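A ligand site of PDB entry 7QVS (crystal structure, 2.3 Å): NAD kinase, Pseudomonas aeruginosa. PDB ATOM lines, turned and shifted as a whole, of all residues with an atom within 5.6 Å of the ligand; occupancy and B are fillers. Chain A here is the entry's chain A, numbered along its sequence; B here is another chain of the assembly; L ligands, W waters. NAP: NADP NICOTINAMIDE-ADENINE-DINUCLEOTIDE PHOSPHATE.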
ATOM      1  N   ARG A  12     -28.879 -11.816   2.213  1.00  0.00           N
ATOM      2  CA  ARG A  12     -29.453 -11.018   3.296  1.00  0.00           C
ATOM      3  C   ARG A  12     -29.489  -9.557   2.851  1.00  0.00           C
ATOM      4  O   ARG A  12     -28.450  -8.911   2.691  1.00  0.00           O
ATOM      5  CB  ARG A  12     -28.668 -11.186   4.588  1.00  0.00           C
ATOM      6  CG  ARG A  12     -29.526 -10.941   5.836  1.00  0.00           C
ATOM      7  CD  ARG A  12     -29.040 -11.701   7.065  1.00  0.00           C
ATOM      8  NE  ARG A  12     -27.640 -11.418   7.374  1.00  0.00           N
ATOM      9  CZ  ARG A  12     -27.161 -11.229   8.592  1.00  0.00           C
ATOM     10  NH1 ARG A  12     -27.947 -11.221   9.662  1.00  0.00           N
ATOM     11  NH2 ARG A  12     -25.849 -11.058   8.752  1.00  0.00           N
ATOM     12  N   GLY A  70     -23.618 -12.680   1.513  1.00  0.00           N
ATOM     13  CA  GLY A  70     -23.842 -11.865   2.684  1.00  0.00           C
ATOM     14  C   GLY A  70     -23.223 -12.320   3.999  1.00  0.00           C
ATOM     15  O   GLY A  70     -23.635 -11.848   5.059  1.00  0.00           O
ATOM     16  N   GLY A  71     -22.256 -13.221   3.955  1.00  0.00           N
ATOM     17  CA  GLY A  71     -21.491 -13.532   5.156  1.00  0.00           C
ATOM     18  C   GLY A  71     -22.064 -14.592   6.077  1.00  0.00           C
ATOM     19  O   GLY A  71     -23.085 -15.240   5.808  1.00  0.00           O
ATOM     20  N   ASP A  72     -21.363 -14.761   7.212  1.00  0.00           N
ATOM     21  CA  ASP A  72     -21.653 -15.858   8.141  1.00  0.00           C
ATOM     22  C   ASP A  72     -23.076 -15.774   8.679  1.00  0.00           C
ATOM     23  O   ASP A  72     -23.808 -16.765   8.701  1.00  0.00           O
ATOM     24  CB  ASP A  72     -20.641 -15.841   9.296  1.00  0.00           C
ATOM     25  CG  ASP A  72     -19.311 -16.521   8.928  1.00  0.00           C
ATOM     26  OD1 ASP A  72     -19.239 -17.246   7.911  1.00  0.00           O
ATOM     27  OD2 ASP A  72     -18.327 -16.327   9.678  1.00  0.00           O
ATOM     28  N   GLY A  73     -23.487 -14.595   9.135  1.00  0.00           N
ATOM     29  CA  GLY A  73     -24.840 -14.454   9.654  1.00  0.00           C
ATOM     30  C   GLY A  73     -25.904 -14.862   8.646  1.00  0.00           C
ATOM     31  O   GLY A  73     -26.908 -15.485   9.012  1.00  0.00           O
ATOM     32  N   SER A  74     -25.689 -14.533   7.375  1.00  0.00           N
ATOM     33  CA  SER A  74     -26.620 -14.900   6.317  1.00  0.00           C
ATOM     34  C   SER A  74     -26.566 -16.395   5.986  1.00  0.00           C
ATOM     35  O   SER A  74     -27.570 -16.958   5.529  1.00  0.00           O
ATOM     36  CB  SER A  74     -26.320 -14.081   5.068  1.00  0.00           C
ATOM     37  OG  SER A  74     -27.300 -14.292   4.082  1.00  0.00           O
ATOM     38  N   LEU A  76     -26.421 -18.659   8.260  1.00  0.00           N
ATOM     39  CA  LEU A  76     -27.222 -19.352   9.267  1.00  0.00           C
ATOM     40  C   LEU A  76     -28.678 -19.540   8.806  1.00  0.00           C
ATOM     41  O   LEU A  76     -29.217 -20.644   8.884  1.00  0.00           O
ATOM     42  CB  LEU A  76     -27.180 -18.594  10.603  1.00  0.00           C
ATOM     43  CG  LEU A  76     -25.848 -18.101  11.172  1.00  0.00           C
ATOM     44  CD1 LEU A  76     -26.078 -17.353  12.473  1.00  0.00           C
ATOM     45  CD2 LEU A  76     -24.872 -19.260  11.365  1.00  0.00           C
ATOM     46  N   ARG A  94     -19.014 -11.044   2.487  1.00  0.00           N
ATOM     47  CA  ARG A  94     -19.322  -9.631   2.301  1.00  0.00           C
ATOM     48  C   ARG A  94     -18.083  -8.781   2.060  1.00  0.00           C
ATOM     49  O   ARG A  94     -18.208  -7.633   1.633  1.00  0.00           O
ATOM     50  CB  ARG A  94     -20.085  -9.102   3.522  1.00  0.00           C
ATOM     51  CG  ARG A  94     -21.607  -9.076   3.357  1.00  0.00           C
ATOM     52  CD  ARG A  94     -22.321  -8.789   4.687  1.00  0.00           C
ATOM     53  NE  ARG A  94     -21.573  -7.899   5.557  1.00  0.00           N
ATOM     54  CZ  ARG A  94     -21.385  -8.096   6.860  1.00  0.00           C
ATOM     55  NH1 ARG A  94     -21.843  -9.185   7.466  1.00  0.00           N
ATOM     56  NH2 ARG A  94     -20.722  -7.196   7.565  1.00  0.00           N
ATOM     57  N   PHE A  99     -16.130 -18.040   8.910  1.00  0.00           N
ATOM     58  CA  PHE A  99     -16.068 -19.452   9.248  1.00  0.00           C
ATOM     59  C   PHE A  99     -16.968 -20.293   8.344  1.00  0.00           C
ATOM     60  O   PHE A  99     -16.780 -21.508   8.272  1.00  0.00           O
ATOM     61  CB  PHE A  99     -16.411 -19.663  10.718  1.00  0.00           C
ATOM     62  CG  PHE A  99     -15.273 -19.356  11.630  1.00  0.00           C
ATOM     63  CD1 PHE A  99     -14.292 -20.310  11.867  1.00  0.00           C
ATOM     64  CD2 PHE A  99     -15.144 -18.097  12.180  1.00  0.00           C
ATOM     65  CE1 PHE A  99     -13.205 -20.010  12.677  1.00  0.00           C
ATOM     66  CE2 PHE A  99     -14.064 -17.792  13.001  1.00  0.00           C
ATOM     67  CZ  PHE A  99     -13.095 -18.753  13.242  1.00  0.00           C
ATOM     68  N   LEU A 100     -17.899 -19.664   7.620  1.00  0.00           N
ATOM     69  CA  LEU A 100     -18.788 -20.370   6.720  1.00  0.00           C
ATOM     70  C   LEU A 100     -18.657 -19.978   5.261  1.00  0.00           C
ATOM     71  O   LEU A 100     -19.158 -20.715   4.398  1.00  0.00           O
ATOM     72  CB  LEU A 100     -20.253 -20.183   7.161  1.00  0.00           C
ATOM     73  CG  LEU A 100     -20.452 -20.735   8.585  1.00  0.00           C
ATOM     74  CD1 LEU A 100     -21.741 -20.268   9.231  1.00  0.00           C
ATOM     75  CD2 LEU A 100     -20.375 -22.250   8.516  1.00  0.00           C
ATOM     76  N   ASN A 146     -25.697 -22.210  14.656  1.00  0.00           N
ATOM     77  CA  ASN A 146     -24.737 -21.694  15.650  1.00  0.00           C
ATOM     78  C   ASN A 146     -25.150 -22.086  17.063  1.00  0.00           C
ATOM     79  O   ASN A 146     -24.421 -22.802  17.757  1.00  0.00           O
ATOM     80  CB  ASN A 146     -24.638 -20.164  15.570  1.00  0.00           C
ATOM     81  CG  ASN A 146     -23.549 -19.644  14.607  1.00  0.00           C
ATOM     82  OD1 ASN A 146     -22.830 -20.391  13.953  1.00  0.00           O
ATOM     83  ND2 ASN A 146     -23.443 -18.334  14.539  1.00  0.00           N
ATOM     84  N   ASP A 147     -26.296 -21.558  17.536  1.00  0.00           N
ATOM     85  CA  ASP A 147     -26.553 -21.558  18.968  1.00  0.00           C
ATOM     86  C   ASP A 147     -28.029 -21.341  19.291  1.00  0.00           C
ATOM     87  O   ASP A 147     -28.789 -20.722  18.534  1.00  0.00           O
ATOM     88  CB  ASP A 147     -25.718 -20.484  19.707  1.00  0.00           C
ATOM     89  CG  ASP A 147     -25.586 -19.170  18.928  1.00  0.00           C
ATOM     90  OD1 ASP A 147     -26.579 -18.644  18.355  1.00  0.00           O
ATOM     91  OD2 ASP A 147     -24.469 -18.628  18.912  1.00  0.00           O
ATOM     92  N   THR A 184     -19.943 -25.394  14.968  1.00  0.00           N
ATOM     93  CA  THR A 184     -20.012 -24.205  14.120  1.00  0.00           C
ATOM     94  C   THR A 184     -20.170 -22.938  14.958  1.00  0.00           C
ATOM     95  O   THR A 184     -19.477 -21.937  14.732  1.00  0.00           O
ATOM     96  CB  THR A 184     -21.173 -24.316  13.112  1.00  0.00           C
ATOM     97  OG1 THR A 184     -21.054 -25.525  12.341  1.00  0.00           O
ATOM     98  CG2 THR A 184     -21.183 -23.120  12.174  1.00  0.00           C
ATOM     99  N   GLY A 185     -21.096 -22.953  15.922  1.00  0.00           N
ATOM    100  CA  GLY A 185     -21.350 -21.772  16.735  1.00  0.00           C
ATOM    101  C   GLY A 185     -20.329 -21.499  17.819  1.00  0.00           C
ATOM    102  O   GLY A 185     -20.378 -20.424  18.420  1.00  0.00           O
ATOM    103  N   SER A 186     -19.393 -22.417  18.043  1.00  0.00           N
ATOM    104  CA  SER A 186     -18.407 -22.290  19.109  1.00  0.00           C
ATOM    105  C   SER A 186     -17.505 -21.080  18.911  1.00  0.00           C
ATOM    106  O   SER A 186     -16.960 -20.540  19.878  1.00  0.00           O
ATOM    107  CB  SER A 186     -17.561 -23.562  19.207  1.00  0.00           C
ATOM    108  OG  SER A 186     -16.619 -23.698  18.117  1.00  0.00           O
ATOM    109  N   THR A 187     -17.316 -20.643  17.664  1.00  0.00           N
ATOM    110  CA  THR A 187     -16.519 -19.453  17.384  1.00  0.00           C
ATOM    111  C   THR A 187     -17.357 -18.172  17.373  1.00  0.00           C
ATOM    112  O   THR A 187     -16.825 -17.096  17.131  1.00  0.00           O
ATOM    113  CB  THR A 187     -15.766 -19.620  16.039  1.00  0.00           C
ATOM    114  OG1 THR A 187     -16.692 -19.942  15.003  1.00  0.00           O
ATOM    115  CG2 THR A 187     -14.692 -20.729  16.105  1.00  0.00           C
ATOM    116  N   ALA A 188     -18.653 -18.240  17.652  1.00  0.00           N
ATOM    117  CA  ALA A 188     -19.472 -17.017  17.634  1.00  0.00           C
ATOM    118  C   ALA A 188     -19.765 -16.459  19.050  1.00  0.00           C
ATOM    119  O   ALA A 188     -18.826 -16.095  19.764  1.00  0.00           O
ATOM    120  CB  ALA A 188     -20.761 -17.300  16.861  1.00  0.00           C
ATOM    121  N   TYR A 189     -21.029 -16.371  19.453  1.00  0.00           N
ATOM    122  CA  TYR A 189     -21.386 -15.815  20.763  1.00  0.00           C
ATOM    123  C   TYR A 189     -20.687 -16.574  21.898  1.00  0.00           C
ATOM    124  O   TYR A 189     -20.164 -15.960  22.843  1.00  0.00           O
ATOM    125  CB  TYR A 189     -22.913 -15.856  20.947  1.00  0.00           C
ATOM    126  CG  TYR A 189     -23.540 -14.789  21.839  1.00  0.00           C
ATOM    127  CD1 TYR A 189     -22.781 -13.998  22.704  1.00  0.00           C
ATOM    128  CD2 TYR A 189     -24.928 -14.588  21.820  1.00  0.00           C
ATOM    129  CE1 TYR A 189     -23.390 -13.025  23.528  1.00  0.00           C
ATOM    130  CE2 TYR A 189     -25.540 -13.644  22.608  1.00  0.00           C
ATOM    131  CZ  TYR A 189     -24.766 -12.854  23.468  1.00  0.00           C
ATOM    132  OH  TYR A 189     -25.399 -11.917  24.233  1.00  0.00           O
ATOM    133  N   ALA A 190     -20.640 -17.904  21.818  1.00  0.00           N
ATOM    134  CA  ALA A 190     -19.980 -18.707  22.839  1.00  0.00           C
ATOM    135  C   ALA A 190     -18.509 -18.312  23.039  1.00  0.00           C
ATOM    136  O   ALA A 190     -18.023 -18.277  24.171  1.00  0.00           O
ATOM    137  CB  ALA A 190     -20.122 -20.175  22.460  1.00  0.00           C
ATOM    138  N   SER A 192     -17.099 -15.287  22.480  1.00  0.00           N
ATOM    139  CA  SER A 192     -17.107 -14.008  23.172  1.00  0.00           C
ATOM    140  C   SER A 192     -17.470 -14.148  24.642  1.00  0.00           C
ATOM    141  O   SER A 192     -17.056 -13.321  25.455  1.00  0.00           O
ATOM    142  CB  SER A 192     -18.097 -13.080  22.485  1.00  0.00           C
ATOM    143  OG  SER A 192     -17.742 -12.912  21.138  1.00  0.00           O
ATOM    144  N   ASP A 245     -29.851 -18.849  16.653  1.00  0.00           N
ATOM    145  CA  ASP A 245     -28.963 -18.139  15.742  1.00  0.00           C
ATOM    146  C   ASP A 245     -29.140 -16.610  15.803  1.00  0.00           C
ATOM    147  O   ASP A 245     -28.861 -15.907  14.817  1.00  0.00           O
ATOM    148  CB  ASP A 245     -29.177 -18.631  14.297  1.00  0.00           C
ATOM    149  CG  ASP A 245     -28.586 -20.013  14.060  1.00  0.00           C
ATOM    150  OD1 ASP A 245     -27.784 -20.485  14.907  1.00  0.00           O
ATOM    151  OD2 ASP A 245     -28.938 -20.627  13.028  1.00  0.00           O
ATOM    152  N   GLY A 246     -29.595 -16.085  16.939  1.00  0.00           N
ATOM    153  CA  GLY A 246     -29.868 -14.659  17.058  1.00  0.00           C
ATOM    154  C   GLY A 246     -30.915 -14.117  16.105  1.00  0.00           C
ATOM    155  O   GLY A 246     -31.034 -12.898  15.963  1.00  0.00           O
ATOM    156  N   GLN A 247     -31.680 -14.993  15.453  1.00  0.00           N
ATOM    157  CA  GLN A 247     -32.545 -14.584  14.350  1.00  0.00           C
ATOM    158  C   GLN A 247     -33.983 -15.056  14.485  1.00  0.00           C
ATOM    159  O   GLN A 247     -34.836 -14.537  13.777  1.00  0.00           O
ATOM    160  CB  GLN A 247     -31.979 -15.071  13.007  1.00  0.00           C
ATOM    161  CG  GLN A 247     -30.654 -14.385  12.612  1.00  0.00           C
ATOM    162  CD  GLN A 247     -29.838 -15.155  11.560  1.00  0.00           C
ATOM    163  OE1 GLN A 247     -30.319 -16.125  10.961  1.00  0.00           O
ATOM    164  NE2 GLN A 247     -28.600 -14.719  11.326  1.00  0.00           N
ATOM    165  N   LYS A 284      -8.813 -14.895  11.011  1.00  0.00           N
ATOM    166  CA  LYS A 284      -9.912 -14.250  11.723  1.00  0.00           C
ATOM    167  C   LYS A 284      -9.598 -14.025  13.206  1.00  0.00           C
ATOM    168  O   LYS A 284     -10.096 -13.067  13.801  1.00  0.00           O
ATOM    169  CB  LYS A 284     -11.184 -15.085  11.592  1.00  0.00           C
ATOM    170  CG  LYS A 284     -12.139 -14.646  10.492  1.00  0.00           C
ATOM    171  CD  LYS A 284     -13.537 -15.183  10.763  1.00  0.00           C
ATOM    172  CE  LYS A 284     -14.542 -14.058  11.026  1.00  0.00           C
ATOM    173  NZ  LYS A 284     -15.930 -14.374  10.524  1.00  0.00           N
ATOM    174  N   THR B 156     -31.107  -8.570  19.708  1.00  0.00           N
ATOM    175  CA  THR B 156     -30.183  -9.667  19.966  1.00  0.00           C
ATOM    176  C   THR B 156     -28.934  -9.571  19.109  1.00  0.00           C
ATOM    177  O   THR B 156     -28.294 -10.588  18.839  1.00  0.00           O
ATOM    178  CB  THR B 156     -30.839 -11.024  19.711  1.00  0.00           C
ATOM    179  OG1 THR B 156     -31.387 -11.043  18.391  1.00  0.00           O
ATOM    180  CG2 THR B 156     -31.928 -11.285  20.727  1.00  0.00           C
ATOM    181  N   ARG B 157     -28.615  -8.377  18.622  1.00  0.00           N
ATOM    182  CA  ARG B 157     -27.454  -8.218  17.782  1.00  0.00           C
ATOM    183  C   ARG B 157     -26.374  -7.437  18.520  1.00  0.00           C
ATOM    184  O   ARG B 157     -26.643  -6.790  19.535  1.00  0.00           O
ATOM    185  CB  ARG B 157     -27.847  -7.539  16.473  1.00  0.00           C
ATOM    186  CG  ARG B 157     -28.861  -8.382  15.710  1.00  0.00           C
ATOM    187  CD  ARG B 157     -29.111  -7.885  14.318  1.00  0.00           C
ATOM    188  NE  ARG B 157     -27.991  -8.174  13.433  1.00  0.00           N
ATOM    189  CZ  ARG B 157     -28.079  -8.197  12.107  1.00  0.00           C
ATOM    190  NH1 ARG B 157     -29.223  -7.982  11.484  1.00  0.00           N
ATOM    191  NH2 ARG B 157     -26.983  -8.432  11.397  1.00  0.00           N
ATOM    192  N   MET B 158     -25.153  -7.572  18.058  1.00  0.00           N
ATOM    193  CA  MET B 158     -24.078  -6.786  18.647  1.00  0.00           C
ATOM    194  C   MET B 158     -24.246  -5.314  18.297  1.00  0.00           C
ATOM    195  O   MET B 158     -24.813  -4.959  17.256  1.00  0.00           O
ATOM    196  CB  MET B 158     -22.707  -7.302  18.181  1.00  0.00           C
ATOM    197  CG  MET B 158     -22.264  -8.616  18.860  1.00  0.00           C
ATOM    198  SD  MET B 158     -20.558  -9.081  18.503  1.00  0.00           S
ATOM    199  CE  MET B 158     -20.737  -9.580  16.803  1.00  0.00           C
ATOM    200  N   LYS B 174     -16.994  -3.691  18.578  1.00  0.00           N
ATOM    201  CA  LYS B 174     -18.242  -4.405  18.439  1.00  0.00           C
ATOM    202  C   LYS B 174     -18.364  -5.334  19.638  1.00  0.00           C
ATOM    203  O   LYS B 174     -17.438  -6.095  19.925  1.00  0.00           O
ATOM    204  CB  LYS B 174     -18.255  -5.225  17.145  1.00  0.00           C
ATOM    205  CG  LYS B 174     -19.448  -5.078  16.269  1.00  0.00           C
ATOM    206  CD  LYS B 174     -19.203  -5.706  14.886  1.00  0.00           C
ATOM    207  CE  LYS B 174     -20.375  -6.598  14.469  1.00  0.00           C
ATOM    208  NZ  LYS B 174     -20.151  -7.382  13.207  1.00  0.00           N
ATOM    209  N   ALA B 175     -19.497  -5.269  20.331  1.00  0.00           N
ATOM    210  CA  ALA B 175     -19.725  -6.031  21.562  1.00  0.00           C
ATOM    211  C   ALA B 175     -21.215  -5.952  21.891  1.00  0.00           C
ATOM    212  O   ALA B 175     -21.978  -5.250  21.225  1.00  0.00           O
ATOM    213  CB  ALA B 175     -18.862  -5.486  22.705  1.00  0.00           C
ATOM    214  N   ASP B 176     -21.614  -6.700  22.928  1.00  0.00           N
ATOM    215  CA  ASP B 176     -22.955  -6.490  23.481  1.00  0.00           C
ATOM    216  C   ASP B 176     -23.089  -5.107  24.114  1.00  0.00           C
ATOM    217  O   ASP B 176     -24.185  -4.537  24.153  1.00  0.00           O
ATOM    218  CB  ASP B 176     -23.279  -7.549  24.528  1.00  0.00           C
ATOM    219  CG  ASP B 176     -23.953  -8.810  23.940  1.00  0.00           C
ATOM    220  OD1 ASP B 176     -23.917  -9.051  22.704  1.00  0.00           O
ATOM    221  OD2 ASP B 176     -24.528  -9.585  24.742  1.00  0.00           O
ATOM    222  N   MET B 210     -18.599  -5.981  27.428  1.00  0.00           N
ATOM    223  CA  MET B 210     -19.569  -7.070  27.539  1.00  0.00           C
ATOM    224  C   MET B 210     -19.567  -7.898  26.269  1.00  0.00           C
ATOM    225  O   MET B 210     -19.978  -7.401  25.208  1.00  0.00           O
ATOM    226  CB  MET B 210     -20.984  -6.560  27.757  1.00  0.00           C
ATOM    227  CG  MET B 210     -21.222  -5.695  28.934  1.00  0.00           C
ATOM    228  SD  MET B 210     -22.983  -5.289  29.039  1.00  0.00           S
ATOM    229  CE  MET B 210     -23.832  -6.586  28.154  1.00  0.00           C
ATOM    230  N   TYR B 211     -19.188  -9.174  26.390  1.00  0.00           N
ATOM    231  CA  TYR B 211     -19.187 -10.121  25.287  1.00  0.00           C
ATOM    232  C   TYR B 211     -18.549  -9.515  24.024  1.00  0.00           C
ATOM    233  O   TYR B 211     -19.220  -9.374  22.992  1.00  0.00           O
ATOM    234  CB  TYR B 211     -20.607 -10.604  24.978  1.00  0.00           C
ATOM    235  CG  TYR B 211     -21.335 -11.132  26.184  1.00  0.00           C
ATOM    236  CD1 TYR B 211     -21.047 -12.398  26.724  1.00  0.00           C
ATOM    237  CD2 TYR B 211     -22.297 -10.346  26.823  1.00  0.00           C
ATOM    238  CE1 TYR B 211     -21.712 -12.863  27.854  1.00  0.00           C
ATOM    239  CE2 TYR B 211     -22.965 -10.798  27.946  1.00  0.00           C
ATOM    240  CZ  TYR B 211     -22.675 -12.057  28.455  1.00  0.00           C
ATOM    241  OH  TYR B 211     -23.356 -12.459  29.583  1.00  0.00           O
ATOM    242  N   PRO B 212     -17.294  -9.089  24.101  1.00  0.00           N
ATOM    243  CA  PRO B 212     -16.687  -8.397  22.955  1.00  0.00           C
ATOM    244  C   PRO B 212     -16.406  -9.346  21.792  1.00  0.00           C
ATOM    245  O   PRO B 212     -16.047 -10.508  21.989  1.00  0.00           O
ATOM    246  CB  PRO B 212     -15.393  -7.820  23.523  1.00  0.00           C
ATOM    247  CG  PRO B 212     -15.055  -8.732  24.678  1.00  0.00           C
ATOM    248  CD  PRO B 212     -16.379  -9.173  25.246  1.00  0.00           C
ATOM    249  N   HIS B 213     -16.594  -8.819  20.596  1.00  0.00           N
ATOM    250  CA  HIS B 213     -16.177  -9.500  19.368  1.00  0.00           C
ATOM    251  C   HIS B 213     -14.662  -9.722  19.332  1.00  0.00           C
ATOM    252  O   HIS B 213     -14.171 -10.782  18.921  1.00  0.00           O
ATOM    253  CB  HIS B 213     -16.634  -8.659  18.173  1.00  0.00           C
ATOM    254  CG  HIS B 213     -16.658  -9.376  16.861  1.00  0.00           C
ATOM    255  ND1 HIS B 213     -17.447 -10.483  16.618  1.00  0.00           N
ATOM    256  CD2 HIS B 213     -16.019  -9.107  15.695  1.00  0.00           C
ATOM    257  CE1 HIS B 213     -17.278 -10.867  15.369  1.00  0.00           C
ATOM    258  NE2 HIS B 213     -16.413 -10.055  14.792  1.00  0.00           N
HETATM  259  PA  NAP L   1     -24.864 -10.067  14.612  1.00  0.00           P
HETATM  260  O1A NAP L   1     -24.937  -9.851  16.133  1.00  0.00           O
HETATM  261  O2A NAP L   1     -25.264  -8.843  13.865  1.00  0.00           O
HETATM  262  O5B NAP L   1     -23.315 -10.451  14.117  1.00  0.00           O
HETATM  263  C5B NAP L   1     -22.708 -11.649  14.539  1.00  0.00           C
HETATM  264  C4B NAP L   1     -21.251 -11.558  14.041  1.00  0.00           C
HETATM  265  O4B NAP L   1     -20.626 -12.989  14.289  1.00  0.00           O
HETATM  266  C3B NAP L   1     -21.169 -11.312  12.743  1.00  0.00           C
HETATM  267  O3B NAP L   1     -19.897 -10.529  12.520  1.00  0.00           O
HETATM  268  C2B NAP L   1     -21.003 -12.677  12.061  1.00  0.00           C
HETATM  269  O2B NAP L   1     -20.182 -12.619  10.940  1.00  0.00           O
HETATM  270  C1B NAP L   1     -20.230 -13.446  13.115  1.00  0.00           C
HETATM  271  N9A NAP L   1     -20.567 -14.870  13.095  1.00  0.00           N
HETATM  272  C8A NAP L   1     -21.735 -15.424  12.813  1.00  0.00           C
HETATM  273  N7A NAP L   1     -21.606 -16.723  12.914  1.00  0.00           N
HETATM  274  C5A NAP L   1     -20.332 -16.995  13.284  1.00  0.00           C
HETATM  275  C6A NAP L   1     -19.589 -18.163  13.549  1.00  0.00           C
HETATM  276  N6A NAP L   1     -20.209 -19.453  13.461  1.00  0.00           N
HETATM  277  N1A NAP L   1     -18.292 -18.045  13.911  1.00  0.00           N
HETATM  278  C2A NAP L   1     -17.746 -16.886  13.973  1.00  0.00           C
HETATM  279  N3A NAP L   1     -18.406 -15.755  13.723  1.00  0.00           N
HETATM  280  C4A NAP L   1     -19.684 -15.809  13.384  1.00  0.00           C
HETATM  281  O3  NAP L   1     -25.943 -11.269  14.303  1.00  0.00           O
HETATM  282  PN  NAP L   1     -25.960 -12.243  13.010  1.00  0.00           P
HETATM  283  O1N NAP L   1     -25.068 -11.661  11.886  1.00  0.00           O
HETATM  284  O2N NAP L   1     -27.425 -12.348  12.627  1.00  0.00           O
HETATM  285  O5D NAP L   1     -25.445 -13.733  13.502  1.00  0.00           O
HETATM  286  C5D NAP L   1     -26.185 -14.308  14.570  1.00  0.00           C
HETATM  287  C4D NAP L   1     -25.224 -14.881  15.546  1.00  0.00           C
HETATM  288  O4D NAP L   1     -24.489 -13.583  16.173  1.00  0.00           O
HETATM  289  C3D NAP L   1     -25.695 -15.555  16.589  1.00  0.00           C
HETATM  290  O3D NAP L   1     -25.785 -16.989  16.243  1.00  0.00           O
HETATM  291  C2D NAP L   1     -24.622 -15.330  17.706  1.00  0.00           C
HETATM  292  O2D NAP L   1     -23.776 -16.351  17.842  1.00  0.00           O
HETATM  293  C1D NAP L   1     -23.848 -14.049  17.216  1.00  0.00           C
HETATM  294  N1N NAP L   1     -23.899 -13.049  18.323  1.00  0.00           N
HETATM  295  C2N NAP L   1     -22.769 -12.764  18.936  1.00  0.00           C
HETATM  296  C3N NAP L   1     -22.839 -11.855  19.975  1.00  0.00           C
HETATM  297  C7N NAP L   1     -21.575 -11.510  20.719  1.00  0.00           C
HETATM  298  O7N NAP L   1     -20.531 -12.126  20.435  1.00  0.00           O
HETATM  299  N7N NAP L   1     -21.611 -10.517  21.737  1.00  0.00           N
HETATM  300  C4N NAP L   1     -24.049 -11.276  20.366  1.00  0.00           C
HETATM  301  C5N NAP L   1     -25.191 -11.619  19.666  1.00  0.00           C
HETATM  302  C6N NAP L   1     -25.071 -12.535  18.632  1.00  0.00           C
HETATM  303  P2B NAP L   1     -20.682 -11.891   9.498  1.00  0.00           P
HETATM  304  O1X NAP L   1     -22.251 -12.072   9.297  1.00  0.00           O
HETATM  305  O2X NAP L   1     -20.331 -10.446   9.565  1.00  0.00           O
HETATM  306  O3X NAP L   1     -19.996 -12.577   8.366  1.00  0.00           O
HETATM  307  O   HOH W   1     -23.494  -8.184  11.901  1.00  0.00           O
HETATM  308  O   HOH W   2     -26.308  -8.889  21.444  1.00  0.00           O
HETATM  309  O   HOH W   3     -23.566 -10.023  10.220  1.00  0.00           O
HETATM  310  O   HOH W   4     -25.085  -6.030  14.534  1.00  0.00           O
HETATM  311  O   HOH W   5     -16.646 -13.403  13.463  1.00  0.00           O
HETATM  312  O   HOH W   6     -27.688 -11.745  16.468  1.00  0.00           O
HETATM  313  O   HOH W   7     -20.569 -14.000  16.779  1.00  0.00           O
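OD2 of Asp 147 is in hydrogen-bond range of O2D of the ligand, 2.6 Å away.
OG1 of Thr 187 sits at hydrogen-bond distance from N1A of the ligand (2.7 Å).
N of Gly 73 is in hydrogen-bond range of O1X of the ligand.
The backbone NH (N) of Asp 72 is in hydrogen-bond range of an oxygen (O3X) of the ligand (2.8 Å).
The side-chain amide oxygen (OD1) of Asn 146 lies within hydrogen-bond range of a nitrogen (N6A) of the ligand, at 2.8 Å.
O2A of the ligand lies within salt-bridge range of NE of Arg 157 of chain B (2.8 Å).
The guanidinium group (NH1) of Arg 94 is in salt-bridge range of an oxygen (O2X) of the ligand (2.9 Å).
A nitrogen (N6A) of the ligand is in hydrogen-bond range of the backbone carbonyl oxygen (O) of Thr 184 (2.9 Å).
The side-chain carboxylate of Asp 176 of chain B is in hydrogen-bond range of a nitrogen (N7N) of the ligand (2.9 Å).
N7N of the ligand is in hydrogen-bond range of O of Tyr 211 of chain B (2.9 Å).
The side-chain amide nitrogen (NE2) of Gln 247 lies within hydrogen-bond range of an oxygen (O2N) of the ligand.
OG of Ser 192 is in hydrogen-bond range of O7N of the ligand, 3.0 Å away.
The backbone NH (N) of Met 158 of chain B is in hydrogen-bond range of an oxygen (O1A) of the ligand, 3.0 Å away.
N7N of the ligand sits close to SD of Met 158 of chain B (3.7 Å).
N of Tyr 189 sits at hydrogen-bond distance from O2D of the ligand (3.2 Å).
NH1 of Arg 12 lies within salt-bridge range of O2N of the ligand (3.2 Å).
NZ of Lys 174 of chain B is in hydrogen-bond range of O3B of the ligand (3.2 Å).
OG1 of Thr 187 lies within hydrogen-bond range of O of Thr 184 (3.4 Å).
NE2 of Gln 247 sits at hydrogen-bond distance from O of Gly 73 (3.0 Å).
OD2 of Asp 72 lies within hydrogen-bond range of N of Phe 99 (2.9 Å).
The side-chain carboxylate (OD1) of Asp 72 sits at hydrogen-bond distance from the backbone NH (N) of Leu 100, 2.8 Å away.
The side-chain hydroxyl (OH) of Tyr 189 is in hydrogen-bond range of the side-chain carboxylate (OD2) of Asp 176 of chain B, 2.5 Å away.
The side-chain hydroxyl of Ser 192 lies within hydrogen-bond range of the backbone carbonyl oxygen of Pro 212 of chain B, 3.1 Å away.
N of Arg 12 lies close to OG of Ser 74.
The backbone carbonyl oxygen (O) of Lys 174 of chain B is in hydrogen-bond range of the backbone NH (N) of His 213 of chain B (2.9 Å).
Merely in contact with the ligand: Gly 71 (3.7 Å), Leu 76 (3.7 Å), Phe 99 (3.4 Å), Ala 188 (3.3 Å), Asp 245 (3.1 Å), Gly 246 (3.95 Å), Thr 156 of chain B (3.4 Å) and His 213 of chain B (3.9 Å).
Within 4 Å of the ligand: Arg 12, Gly 71, Asp 72, Gly 73, Leu 76, Arg 94, Phe 99, Asn 146, Asp 147, Thr 184, Thr 187, Ala 188, Tyr 189, Ser 192, Asp 245, Gly 246, Gln 247, Thr 156 of chain B, Arg 157 of chain B, Met 158 of chain B, Lys 174 of chain B, Asp 176 of chain B, Tyr 211 of chain B and His 213 of chain B.
The nearest printed residue that does not touch the ligand is Gly 185 (4.2 Å).
Water W3 lies within hydrogen-bond range of O1X of the ligand (2.6 Å), NH2 of Arg 12 (2.9 Å) and NH1 of Arg 94 (3.4 Å).
Water W6 bridges the backbone carbonyl oxygen of Thr 156 of chain B (2.7 Å) and an oxygen (O3) of the ligand (2.8 Å).
Water W4 lies within hydrogen-bond range of O2A of the ligand (2.9 Å) and O of Met 158 of chain B (2.9 Å).
Water W5 bridges a nitrogen (N3A) of the ligand (2.9 Å) and the side-chain amino group (NZ) of Lys 284 (3.2 Å).
Water W2 lies within hydrogen-bond range of the side-chain carboxylate of Asp 176 of chain B (2.7 Å) and the backbone carbonyl oxygen of Arg 157 of chain B (2.9 Å).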
